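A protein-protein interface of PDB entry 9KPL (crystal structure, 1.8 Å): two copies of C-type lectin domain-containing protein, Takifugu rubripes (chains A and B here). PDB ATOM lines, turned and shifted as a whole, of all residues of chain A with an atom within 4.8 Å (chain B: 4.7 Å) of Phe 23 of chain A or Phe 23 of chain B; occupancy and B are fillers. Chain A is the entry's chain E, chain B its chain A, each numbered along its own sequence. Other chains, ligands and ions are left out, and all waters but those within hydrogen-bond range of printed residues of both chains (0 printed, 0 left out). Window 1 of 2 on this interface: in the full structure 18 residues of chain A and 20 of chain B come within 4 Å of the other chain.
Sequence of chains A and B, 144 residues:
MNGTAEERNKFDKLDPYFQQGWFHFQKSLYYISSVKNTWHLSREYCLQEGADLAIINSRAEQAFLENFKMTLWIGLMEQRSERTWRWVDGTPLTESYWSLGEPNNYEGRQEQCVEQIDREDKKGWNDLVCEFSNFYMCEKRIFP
Among the printed residues, merely in contact across the chains: Phe 18 of chain A with Phe 25 of chain B, Phe 25 of chain A with Phe 18 of chain B, Phe 25 of chain A with Trp 22 of chain B, Phe 68 of chain A with Phe 68 of chain B, His 24 of chain A with Phe 18 of chain B, Trp 22 of chain A with Phe 25 of chain B, His 24 of chain A with Phe 23 of chain B, Phe 18 of chain A with His 24 of chain B, Phe 23 of chain A with His 24 of chain B, Phe 23 of chain A with Phe 64 of chain B, Phe 68 of chain A with Phe 23 of chain B, Phe 23 of chain A with Phe 23 of chain B, Phe 23 of chain A with Phe 68 of chain B, Phe 64 of chain A with Phe 23 of chain B and Phe 68 of chain A with Ile 32 of chain B.
Phe 18 of chain A touches His 24 of chain B, and with the chains exchanged His 24 of chain A touches Phe 18 of chain B.
Phe 18 of chain A touches Phe 25 of chain B, and with the chains exchanged Phe 25 of chain A touches Phe 18 of chain B.
Trp 22 of chain A touches Phe 25 of chain B, and with the chains exchanged Phe 25 of chain A touches Trp 22 of chain B.
Phe 68 of chain A touches Ile 32 of chain B, but with the chains exchanged Ile 32 of chain A does not touch Phe 68 of chain B (4.01 Å).
ND1 of His 24 of chain B lies within hydrogen-bond range of ND1 of His 24 of chain A, at 2.8 Å.
O of Phe 23 of chain B is in hydrogen-bond range of N of Tyr 30 of chain B, 2.8 Å away.
N of Tyr 30 of chain A is in hydrogen-bond range of O of Phe 23 of chain A, at 2.7 Å.
Hydrophobic or aromatic side chains of chain B within 4 Å of the printed part of chain A: Phe 18, Phe 23, His 24, Phe 25, Ile 32, Phe 64 and Phe 68.
Hydrophobic or aromatic side chains of chain A that line the printed part of chain B: Phe 18, Phe 23, His 24, Phe 25, Phe 64 and Phe 68.
Among the printed residues, 16 pairs touch across the chains.
Among the printed residues, no Asp or Glu carboxylate lies within 4 Å of a Lys or Arg side-chain nitrogen of the other chain.
Printed residues of chain B within 4 Å of Phe 64 of chain A: Phe 23 (3.9 Å).
Of the printed residues of chain A, Phe 23 of chain B touches Phe 23, His 24, Phe 64 and Phe 68.
Leu 29 of chain B touches none of the printed residues of chain A.
Of the printed residues of chain A, Phe 68 of chain B touches Phe 23 and Phe 68.
The nearest residue of chain A that does not touch Phe 23 of chain B is Phe 25 of chain A (4.3 Å).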
ATOM      1  N   PHE A  18     -25.215  14.273  19.593  1.00  0.00           N
ATOM      2  CA  PHE A  18     -24.947  12.926  19.039  1.00  0.00           C
ATOM      3  C   PHE A  18     -25.629  11.827  19.874  1.00  0.00           C
ATOM      4  O   PHE A  18     -26.132  10.829  19.329  1.00  0.00           O
ATOM      5  CB  PHE A  18     -23.457  12.605  19.065  1.00  0.00           C
ATOM      6  CG  PHE A  18     -22.610  13.364  18.062  1.00  0.00           C
ATOM      7  CD1 PHE A  18     -23.131  13.799  16.826  1.00  0.00           C
ATOM      8  CD2 PHE A  18     -21.262  13.612  18.376  1.00  0.00           C
ATOM      9  CE1 PHE A  18     -22.336  14.474  15.914  1.00  0.00           C
ATOM     10  CE2 PHE A  18     -20.433  14.265  17.458  1.00  0.00           C
ATOM     11  CZ  PHE A  18     -20.997  14.722  16.209  1.00  0.00           C
ATOM     12  N   GLY A  21     -28.984  11.370  18.546  1.00  0.00           N
ATOM     13  CA  GLY A  21     -29.179  11.001  17.161  1.00  0.00           C
ATOM     14  C   GLY A  21     -28.962  12.124  16.161  1.00  0.00           C
ATOM     15  O   GLY A  21     -29.151  11.914  14.967  1.00  0.00           O
ATOM     16  N   TRP A  22     -28.561  13.298  16.613  1.00  0.00           N
ATOM     17  CA  TRP A  22     -28.199  14.372  15.680  1.00  0.00           C
ATOM     18  C   TRP A  22     -26.873  14.056  15.042  1.00  0.00           C
ATOM     19  O   TRP A  22     -26.064  13.320  15.613  1.00  0.00           O
ATOM     20  CB  TRP A  22     -28.008  15.716  16.398  1.00  0.00           C
ATOM     21  CG  TRP A  22     -29.270  16.259  16.984  1.00  0.00           C
ATOM     22  CD1 TRP A  22     -29.926  15.796  18.099  1.00  0.00           C
ATOM     23  CD2 TRP A  22     -30.007  17.402  16.518  1.00  0.00           C
ATOM     24  NE1 TRP A  22     -31.054  16.547  18.316  1.00  0.00           N
ATOM     25  CE2 TRP A  22     -31.126  17.547  17.370  1.00  0.00           C
ATOM     26  CE3 TRP A  22     -29.850  18.290  15.436  1.00  0.00           C
ATOM     27  CZ2 TRP A  22     -32.077  18.591  17.209  1.00  0.00           C
ATOM     28  CZ3 TRP A  22     -30.792  19.310  15.249  1.00  0.00           C
ATOM     29  CH2 TRP A  22     -31.897  19.458  16.143  1.00  0.00           C
ATOM     30  N   PHE A  23     -26.624  14.640  13.874  1.00  0.00           N
ATOM     31  CA  PHE A  23     -25.316  14.428  13.238  1.00  0.00           C
ATOM     32  C   PHE A  23     -24.845  15.717  12.581  1.00  0.00           C
ATOM     33  O   PHE A  23     -25.607  16.674  12.379  1.00  0.00           O
ATOM     34  CB  PHE A  23     -25.330  13.218  12.228  1.00  0.00           C
ATOM     35  CG  PHE A  23     -26.485  13.234  11.265  1.00  0.00           C
ATOM     36  CD1 PHE A  23     -27.712  12.664  11.632  1.00  0.00           C
ATOM     37  CD2 PHE A  23     -26.383  13.892  10.004  1.00  0.00           C
ATOM     38  CE1 PHE A  23     -28.817  12.740  10.699  1.00  0.00           C
ATOM     39  CE2 PHE A  23     -27.471  13.916   9.093  1.00  0.00           C
ATOM     40  CZ  PHE A  23     -28.660  13.325   9.442  1.00  0.00           C
ATOM     41  N   HIS A  24     -23.552  15.759  12.280  1.00  0.00           N
ATOM     42  CA  HIS A  24     -22.844  17.009  12.006  1.00  0.00           C
ATOM     43  C   HIS A  24     -22.424  17.098  10.541  1.00  0.00           C
ATOM     44  O   HIS A  24     -21.766  16.191   9.987  1.00  0.00           O
ATOM     45  CB  HIS A  24     -21.615  17.104  12.955  1.00  0.00           C
ATOM     46  CG  HIS A  24     -20.642  18.193  12.611  1.00  0.00           C
ATOM     47  ND1 HIS A  24     -19.287  18.087  12.887  1.00  0.00           N
ATOM     48  CD2 HIS A  24     -20.822  19.424  12.059  1.00  0.00           C
ATOM     49  CE1 HIS A  24     -18.673  19.186  12.480  1.00  0.00           C
ATOM     50  NE2 HIS A  24     -19.580  20.012  11.972  1.00  0.00           N
ATOM     51  N   PHE A  25     -22.785  18.216   9.897  1.00  0.00           N
ATOM     52  CA  PHE A  25     -22.372  18.431   8.508  1.00  0.00           C
ATOM     53  C   PHE A  25     -22.031  19.916   8.388  1.00  0.00           C
ATOM     54  O   PHE A  25     -22.862  20.771   8.709  1.00  0.00           O
ATOM     55  CB  PHE A  25     -23.484  17.997   7.510  1.00  0.00           C
ATOM     56  CG  PHE A  25     -23.168  18.297   6.069  1.00  0.00           C
ATOM     57  CD1 PHE A  25     -22.259  17.534   5.341  1.00  0.00           C
ATOM     58  CD2 PHE A  25     -23.796  19.389   5.406  1.00  0.00           C
ATOM     59  CE1 PHE A  25     -21.918  17.856   4.010  1.00  0.00           C
ATOM     60  CE2 PHE A  25     -23.487  19.681   4.048  1.00  0.00           C
ATOM     61  CZ  PHE A  25     -22.559  18.933   3.335  1.00  0.00           C
ATOM     62  N   SER A  28     -23.335  22.763  10.917  1.00  0.00           N
ATOM     63  CA  SER A  28     -24.611  22.533  11.560  1.00  0.00           C
ATOM     64  C   SER A  28     -24.743  21.108  12.094  1.00  0.00           C
ATOM     65  O   SER A  28     -24.120  20.169  11.600  1.00  0.00           O
ATOM     66  CB  SER A  28     -25.756  22.778  10.560  1.00  0.00           C
ATOM     67  OG  SER A  28     -25.770  24.168  10.147  1.00  0.00           O
ATOM     68  N   LEU A  29     -25.646  20.961  13.031  1.00  0.00           N
ATOM     69  CA  LEU A  29     -26.186  19.652  13.364  1.00  0.00           C
ATOM     70  C   LEU A  29     -27.566  19.458  12.722  1.00  0.00           C
ATOM     71  O   LEU A  29     -28.355  20.425  12.621  1.00  0.00           O
ATOM     72  CB  LEU A  29     -26.314  19.545  14.870  1.00  0.00           C
ATOM     73  CG  LEU A  29     -24.954  19.413  15.568  1.00  0.00           C
ATOM     74  CD1 LEU A  29     -25.250  19.662  17.046  1.00  0.00           C
ATOM     75  CD2 LEU A  29     -24.469  17.951  15.317  1.00  0.00           C
ATOM     76  N   TYR A  30     -27.871  18.200  12.352  1.00  0.00           N
ATOM     77  CA  TYR A  30     -29.127  17.861  11.679  1.00  0.00           C
ATOM     78  C   TYR A  30     -29.781  16.714  12.448  1.00  0.00           C
ATOM     79  O   TYR A  30     -29.105  15.912  13.115  1.00  0.00           O
ATOM     80  CB  TYR A  30     -28.925  17.481  10.230  1.00  0.00           C
ATOM     81  CG  TYR A  30     -28.286  18.566   9.397  1.00  0.00           C
ATOM     82  CD1 TYR A  30     -26.905  18.756   9.422  1.00  0.00           C
ATOM     83  CD2 TYR A  30     -29.051  19.423   8.630  1.00  0.00           C
ATOM     84  CE1 TYR A  30     -26.305  19.764   8.608  1.00  0.00           C
ATOM     85  CE2 TYR A  30     -28.470  20.409   7.812  1.00  0.00           C
ATOM     86  CZ  TYR A  30     -27.095  20.598   7.852  1.00  0.00           C
ATOM     87  OH  TYR A  30     -26.505  21.598   7.087  1.00  0.00           O
ATOM     88  N   ILE A  32     -33.075  13.954  11.814  1.00  0.00           N
ATOM     89  CA  ILE A  32     -34.136  13.398  10.968  1.00  0.00           C
ATOM     90  C   ILE A  32     -35.155  12.771  11.894  1.00  0.00           C
ATOM     91  O   ILE A  32     -34.767  11.961  12.749  1.00  0.00           O
ATOM     92  CB  ILE A  32     -33.561  12.355   9.991  1.00  0.00           C
ATOM     93  CG1 ILE A  32     -32.724  13.047   8.942  1.00  0.00           C
ATOM     94  CG2 ILE A  32     -34.673  11.484   9.335  1.00  0.00           C
ATOM     95  CD1 ILE A  32     -31.891  12.021   8.119  1.00  0.00           C
ATOM     96  N   PHE A  64     -26.381  16.968   0.103  1.00  0.00           N
ATOM     97  CA  PHE A  64     -26.443  16.280   1.391  1.00  0.00           C
ATOM     98  C   PHE A  64     -27.882  15.877   1.697  1.00  0.00           C
ATOM     99  O   PHE A  64     -28.162  14.717   2.027  1.00  0.00           O
ATOM    100  CB  PHE A  64     -25.792  17.221   2.459  1.00  0.00           C
ATOM    101  CG  PHE A  64     -26.047  16.883   3.912  1.00  0.00           C
ATOM    102  CD1 PHE A  64     -25.360  15.820   4.549  1.00  0.00           C
ATOM    103  CD2 PHE A  64     -26.929  17.677   4.668  1.00  0.00           C
ATOM    104  CE1 PHE A  64     -25.582  15.548   5.893  1.00  0.00           C
ATOM    105  CE2 PHE A  64     -27.150  17.461   6.022  1.00  0.00           C
ATOM    106  CZ  PHE A  64     -26.467  16.334   6.649  1.00  0.00           C
ATOM    107  N   PHE A  68     -30.256  11.524   1.349  1.00  0.00           N
ATOM    108  CA  PHE A  68     -30.926  10.690   2.339  1.00  0.00           C
ATOM    109  C   PHE A  68     -32.069   9.910   1.714  1.00  0.00           C
ATOM    110  O   PHE A  68     -32.577   9.007   2.376  1.00  0.00           O
ATOM    111  CB  PHE A  68     -31.395  11.531   3.547  1.00  0.00           C
ATOM    112  CG  PHE A  68     -30.203  12.028   4.356  1.00  0.00           C
ATOM    113  CD1 PHE A  68     -29.307  11.071   4.896  1.00  0.00           C
ATOM    114  CD2 PHE A  68     -29.930  13.399   4.494  1.00  0.00           C
ATOM    115  CE1 PHE A  68     -28.097  11.458   5.582  1.00  0.00           C
ATOM    116  CE2 PHE A  68     -28.806  13.805   5.239  1.00  0.00           C
ATOM    117  CZ  PHE A  68     -27.898  12.852   5.778  1.00  0.00           C
ATOM    118  N   MET A 137     -36.677  17.326   8.784  1.00  0.00           N
ATOM    119  CA  MET A 137     -35.270  17.495   9.134  1.00  0.00           C
ATOM    120  C   MET A 137     -35.102  18.828   9.870  1.00  0.00           C
ATOM    121  O   MET A 137     -35.471  19.883   9.346  1.00  0.00           O
ATOM    122  CB  MET A 137     -34.354  17.483   7.870  1.00  0.00           C
ATOM    123  CG  MET A 137     -32.835  17.831   8.174  1.00  0.00           C
ATOM    124  SD  MET A 137     -31.882  17.842   6.639  1.00  0.00           S
ATOM    125  CE  MET A 137     -31.361  16.100   6.715  1.00  0.00           C
ATOM    126  N   PHE B  18     -16.731  16.678   4.091  1.00  0.00           N
ATOM    127  CA  PHE B  18     -18.037  17.315   3.946  1.00  0.00           C
ATOM    128  C   PHE B  18     -18.247  17.755   2.498  1.00  0.00           C
ATOM    129  O   PHE B  18     -19.352  17.614   1.921  1.00  0.00           O
ATOM    130  CB  PHE B  18     -18.131  18.558   4.850  1.00  0.00           C
ATOM    131  CG  PHE B  18     -18.166  18.287   6.348  1.00  0.00           C
ATOM    132  CD1 PHE B  18     -18.771  17.125   6.891  1.00  0.00           C
ATOM    133  CD2 PHE B  18     -17.623  19.242   7.216  1.00  0.00           C
ATOM    134  CE1 PHE B  18     -18.830  16.949   8.266  1.00  0.00           C
ATOM    135  CE2 PHE B  18     -17.680  19.069   8.586  1.00  0.00           C
ATOM    136  CZ  PHE B  18     -18.269  17.927   9.125  1.00  0.00           C
ATOM    137  N   GLY B  21     -19.758  15.038   0.537  1.00  0.00           N
ATOM    138  CA  GLY B  21     -21.018  14.447   0.977  1.00  0.00           C
ATOM    139  C   GLY B  21     -20.898  13.528   2.187  1.00  0.00           C
ATOM    140  O   GLY B  21     -21.903  12.925   2.577  1.00  0.00           O
ATOM    141  N   TRP B  22     -19.720  13.437   2.825  1.00  0.00           N
ATOM    142  CA  TRP B  22     -19.617  12.691   4.093  1.00  0.00           C
ATOM    143  C   TRP B  22     -20.212  13.505   5.202  1.00  0.00           C
ATOM    144  O   TRP B  22     -20.276  14.741   5.117  1.00  0.00           O
ATOM    145  CB  TRP B  22     -18.136  12.404   4.467  1.00  0.00           C
ATOM    146  CG  TRP B  22     -17.461  11.543   3.475  1.00  0.00           C
ATOM    147  CD1 TRP B  22     -17.059  11.893   2.198  1.00  0.00           C
ATOM    148  CD2 TRP B  22     -17.057  10.175   3.678  1.00  0.00           C
ATOM    149  NE1 TRP B  22     -16.461  10.785   1.574  1.00  0.00           N
ATOM    150  CE2 TRP B  22     -16.439   9.732   2.467  1.00  0.00           C
ATOM    151  CE3 TRP B  22     -17.154   9.286   4.765  1.00  0.00           C
ATOM    152  CZ2 TRP B  22     -15.903   8.441   2.328  1.00  0.00           C
ATOM    153  CZ3 TRP B  22     -16.629   7.979   4.624  1.00  0.00           C
ATOM    154  CH2 TRP B  22     -16.020   7.575   3.412  1.00  0.00           C
ATOM    155  N   PHE B  23     -20.588  12.833   6.295  1.00  0.00           N
ATOM    156  CA  PHE B  23     -21.021  13.583   7.478  1.00  0.00           C
ATOM    157  C   PHE B  23     -20.526  12.869   8.732  1.00  0.00           C
ATOM    158  O   PHE B  23     -20.108  11.706   8.699  1.00  0.00           O
ATOM    159  CB  PHE B  23     -22.566  13.782   7.538  1.00  0.00           C
ATOM    160  CG  PHE B  23     -23.337  12.517   7.215  1.00  0.00           C
ATOM    161  CD1 PHE B  23     -23.559  12.144   5.884  1.00  0.00           C
ATOM    162  CD2 PHE B  23     -23.798  11.681   8.254  1.00  0.00           C
ATOM    163  CE1 PHE B  23     -24.238  10.936   5.578  1.00  0.00           C
ATOM    164  CE2 PHE B  23     -24.490  10.493   7.959  1.00  0.00           C
ATOM    165  CZ  PHE B  23     -24.722  10.136   6.615  1.00  0.00           C
ATOM    166  N   HIS B  24     -20.525  13.619   9.828  1.00  0.00           N
ATOM    167  CA  HIS B  24     -19.779  13.303  11.046  1.00  0.00           C
ATOM    168  C   HIS B  24     -20.727  12.904  12.165  1.00  0.00           C
ATOM    169  O   HIS B  24     -21.667  13.635  12.498  1.00  0.00           O
ATOM    170  CB  HIS B  24     -18.920  14.554  11.446  1.00  0.00           C
ATOM    171  CG  HIS B  24     -18.305  14.481  12.826  1.00  0.00           C
ATOM    172  ND1 HIS B  24     -18.131  15.595  13.642  1.00  0.00           N
ATOM    173  CD2 HIS B  24     -17.841  13.419  13.537  1.00  0.00           C
ATOM    174  CE1 HIS B  24     -17.594  15.223  14.791  1.00  0.00           C
ATOM    175  NE2 HIS B  24     -17.397  13.904  14.747  1.00  0.00           N
ATOM    176  N   PHE B  25     -20.473  11.743  12.769  1.00  0.00           N
ATOM    177  CA  PHE B  25     -21.187  11.328  13.967  1.00  0.00           C
ATOM    178  C   PHE B  25     -20.183  10.668  14.914  1.00  0.00           C
ATOM    179  O   PHE B  25     -19.518   9.729  14.518  1.00  0.00           O
ATOM    180  CB  PHE B  25     -22.333  10.356  13.551  1.00  0.00           C
ATOM    181  CG  PHE B  25     -23.057   9.742  14.722  1.00  0.00           C
ATOM    182  CD1 PHE B  25     -24.059  10.461  15.399  1.00  0.00           C
ATOM    183  CD2 PHE B  25     -22.732   8.457  15.163  1.00  0.00           C
ATOM    184  CE1 PHE B  25     -24.703   9.929  16.509  1.00  0.00           C
ATOM    185  CE2 PHE B  25     -23.383   7.914  16.301  1.00  0.00           C
ATOM    186  CZ  PHE B  25     -24.387   8.640  16.975  1.00  0.00           C
ATOM    187  N   SER B  28     -16.549   9.507  13.867  1.00  0.00           N
ATOM    188  CA  SER B  28     -16.398   8.931  12.533  1.00  0.00           C
ATOM    189  C   SER B  28     -17.031   9.836  11.482  1.00  0.00           C
ATOM    190  O   SER B  28     -17.962  10.575  11.774  1.00  0.00           O
ATOM    191  CB  SER B  28     -17.108   7.557  12.422  1.00  0.00           C
ATOM    192  OG  SER B  28     -16.303   6.581  13.125  1.00  0.00           O
ATOM    193  N   LEU B  29     -16.594   9.633  10.252  1.00  0.00           N
ATOM    194  CA  LEU B  29     -17.299  10.118   9.074  1.00  0.00           C
ATOM    195  C   LEU B  29     -17.997   8.956   8.397  1.00  0.00           C
ATOM    196  O   LEU B  29     -17.491   7.825   8.372  1.00  0.00           O
ATOM    197  CB  LEU B  29     -16.314  10.770   8.102  1.00  0.00           C
ATOM    198  CG  LEU B  29     -15.729  12.121   8.591  1.00  0.00           C
ATOM    199  CD1 LEU B  29     -14.516  12.512   7.757  1.00  0.00           C
ATOM    200  CD2 LEU B  29     -16.817  13.237   8.438  1.00  0.00           C
ATOM    201  N   TYR B  30     -19.146   9.264   7.784  1.00  0.00           N
ATOM    202  CA  TYR B  30     -20.039   8.285   7.185  1.00  0.00           C
ATOM    203  C   TYR B  30     -20.395   8.776   5.799  1.00  0.00           C
ATOM    204  O   TYR B  30     -20.436   9.990   5.565  1.00  0.00           O
ATOM    205  CB  TYR B  30     -21.332   8.093   8.013  1.00  0.00           C
ATOM    206  CG  TYR B  30     -21.057   7.529   9.385  1.00  0.00           C
ATOM    207  CD1 TYR B  30     -20.748   8.360  10.444  1.00  0.00           C
ATOM    208  CD2 TYR B  30     -21.023   6.173   9.592  1.00  0.00           C
ATOM    209  CE1 TYR B  30     -20.539   7.860  11.740  1.00  0.00           C
ATOM    210  CE2 TYR B  30     -20.828   5.626  10.875  1.00  0.00           C
ATOM    211  CZ  TYR B  30     -20.528   6.489  11.932  1.00  0.00           C
ATOM    212  OH  TYR B  30     -20.350   6.025  13.199  1.00  0.00           O
ATOM    213  N   ILE B  32     -23.216   7.687   2.625  1.00  0.00           N
ATOM    214  CA  ILE B  32     -24.307   6.839   2.126  1.00  0.00           C
ATOM    215  C   ILE B  32     -24.234   6.858   0.605  1.00  0.00           C
ATOM    216  O   ILE B  32     -24.180   7.950   0.009  1.00  0.00           O
ATOM    217  CB  ILE B  32     -25.676   7.354   2.626  1.00  0.00           C
ATOM    218  CG1 ILE B  32     -25.746   7.167   4.148  1.00  0.00           C
ATOM    219  CG2 ILE B  32     -26.869   6.628   1.912  1.00  0.00           C
ATOM    220  CD1 ILE B  32     -26.997   7.794   4.819  1.00  0.00           C
ATOM    221  N   PHE B  64     -28.430   5.576  15.253  1.00  0.00           N
ATOM    222  CA  PHE B  64     -28.069   6.482  14.163  1.00  0.00           C
ATOM    223  C   PHE B  64     -28.260   5.795  12.816  1.00  0.00           C
ATOM    224  O   PHE B  64     -28.869   6.359  11.896  1.00  0.00           O
ATOM    225  CB  PHE B  64     -26.612   6.935  14.430  1.00  0.00           C
ATOM    226  CG  PHE B  64     -25.878   7.532  13.248  1.00  0.00           C
ATOM    227  CD1 PHE B  64     -26.097   8.882  12.882  1.00  0.00           C
ATOM    228  CD2 PHE B  64     -24.888   6.775  12.575  1.00  0.00           C
ATOM    229  CE1 PHE B  64     -25.363   9.476  11.854  1.00  0.00           C
ATOM    230  CE2 PHE B  64     -24.170   7.302  11.510  1.00  0.00           C
ATOM    231  CZ  PHE B  64     -24.415   8.694  11.133  1.00  0.00           C
ATOM    232  N   PHE B  68     -31.917   6.307   9.453  1.00  0.00           N
ATOM    233  CA  PHE B  68     -31.879   6.677   8.037  1.00  0.00           C
ATOM    234  C   PHE B  68     -32.995   6.004   7.264  1.00  0.00           C
ATOM    235  O   PHE B  68     -33.226   6.396   6.108  1.00  0.00           O
ATOM    236  CB  PHE B  68     -30.512   6.375   7.373  1.00  0.00           C
ATOM    237  CG  PHE B  68     -29.443   7.281   7.916  1.00  0.00           C
ATOM    238  CD1 PHE B  68     -29.606   8.671   7.781  1.00  0.00           C
ATOM    239  CD2 PHE B  68     -28.406   6.789   8.668  1.00  0.00           C
ATOM    240  CE1 PHE B  68     -28.707   9.600   8.424  1.00  0.00           C
ATOM    241  CE2 PHE B  68     -27.481   7.672   9.228  1.00  0.00           C
ATOM    242  CZ  PHE B  68     -27.646   9.080   9.100  1.00  0.00           C
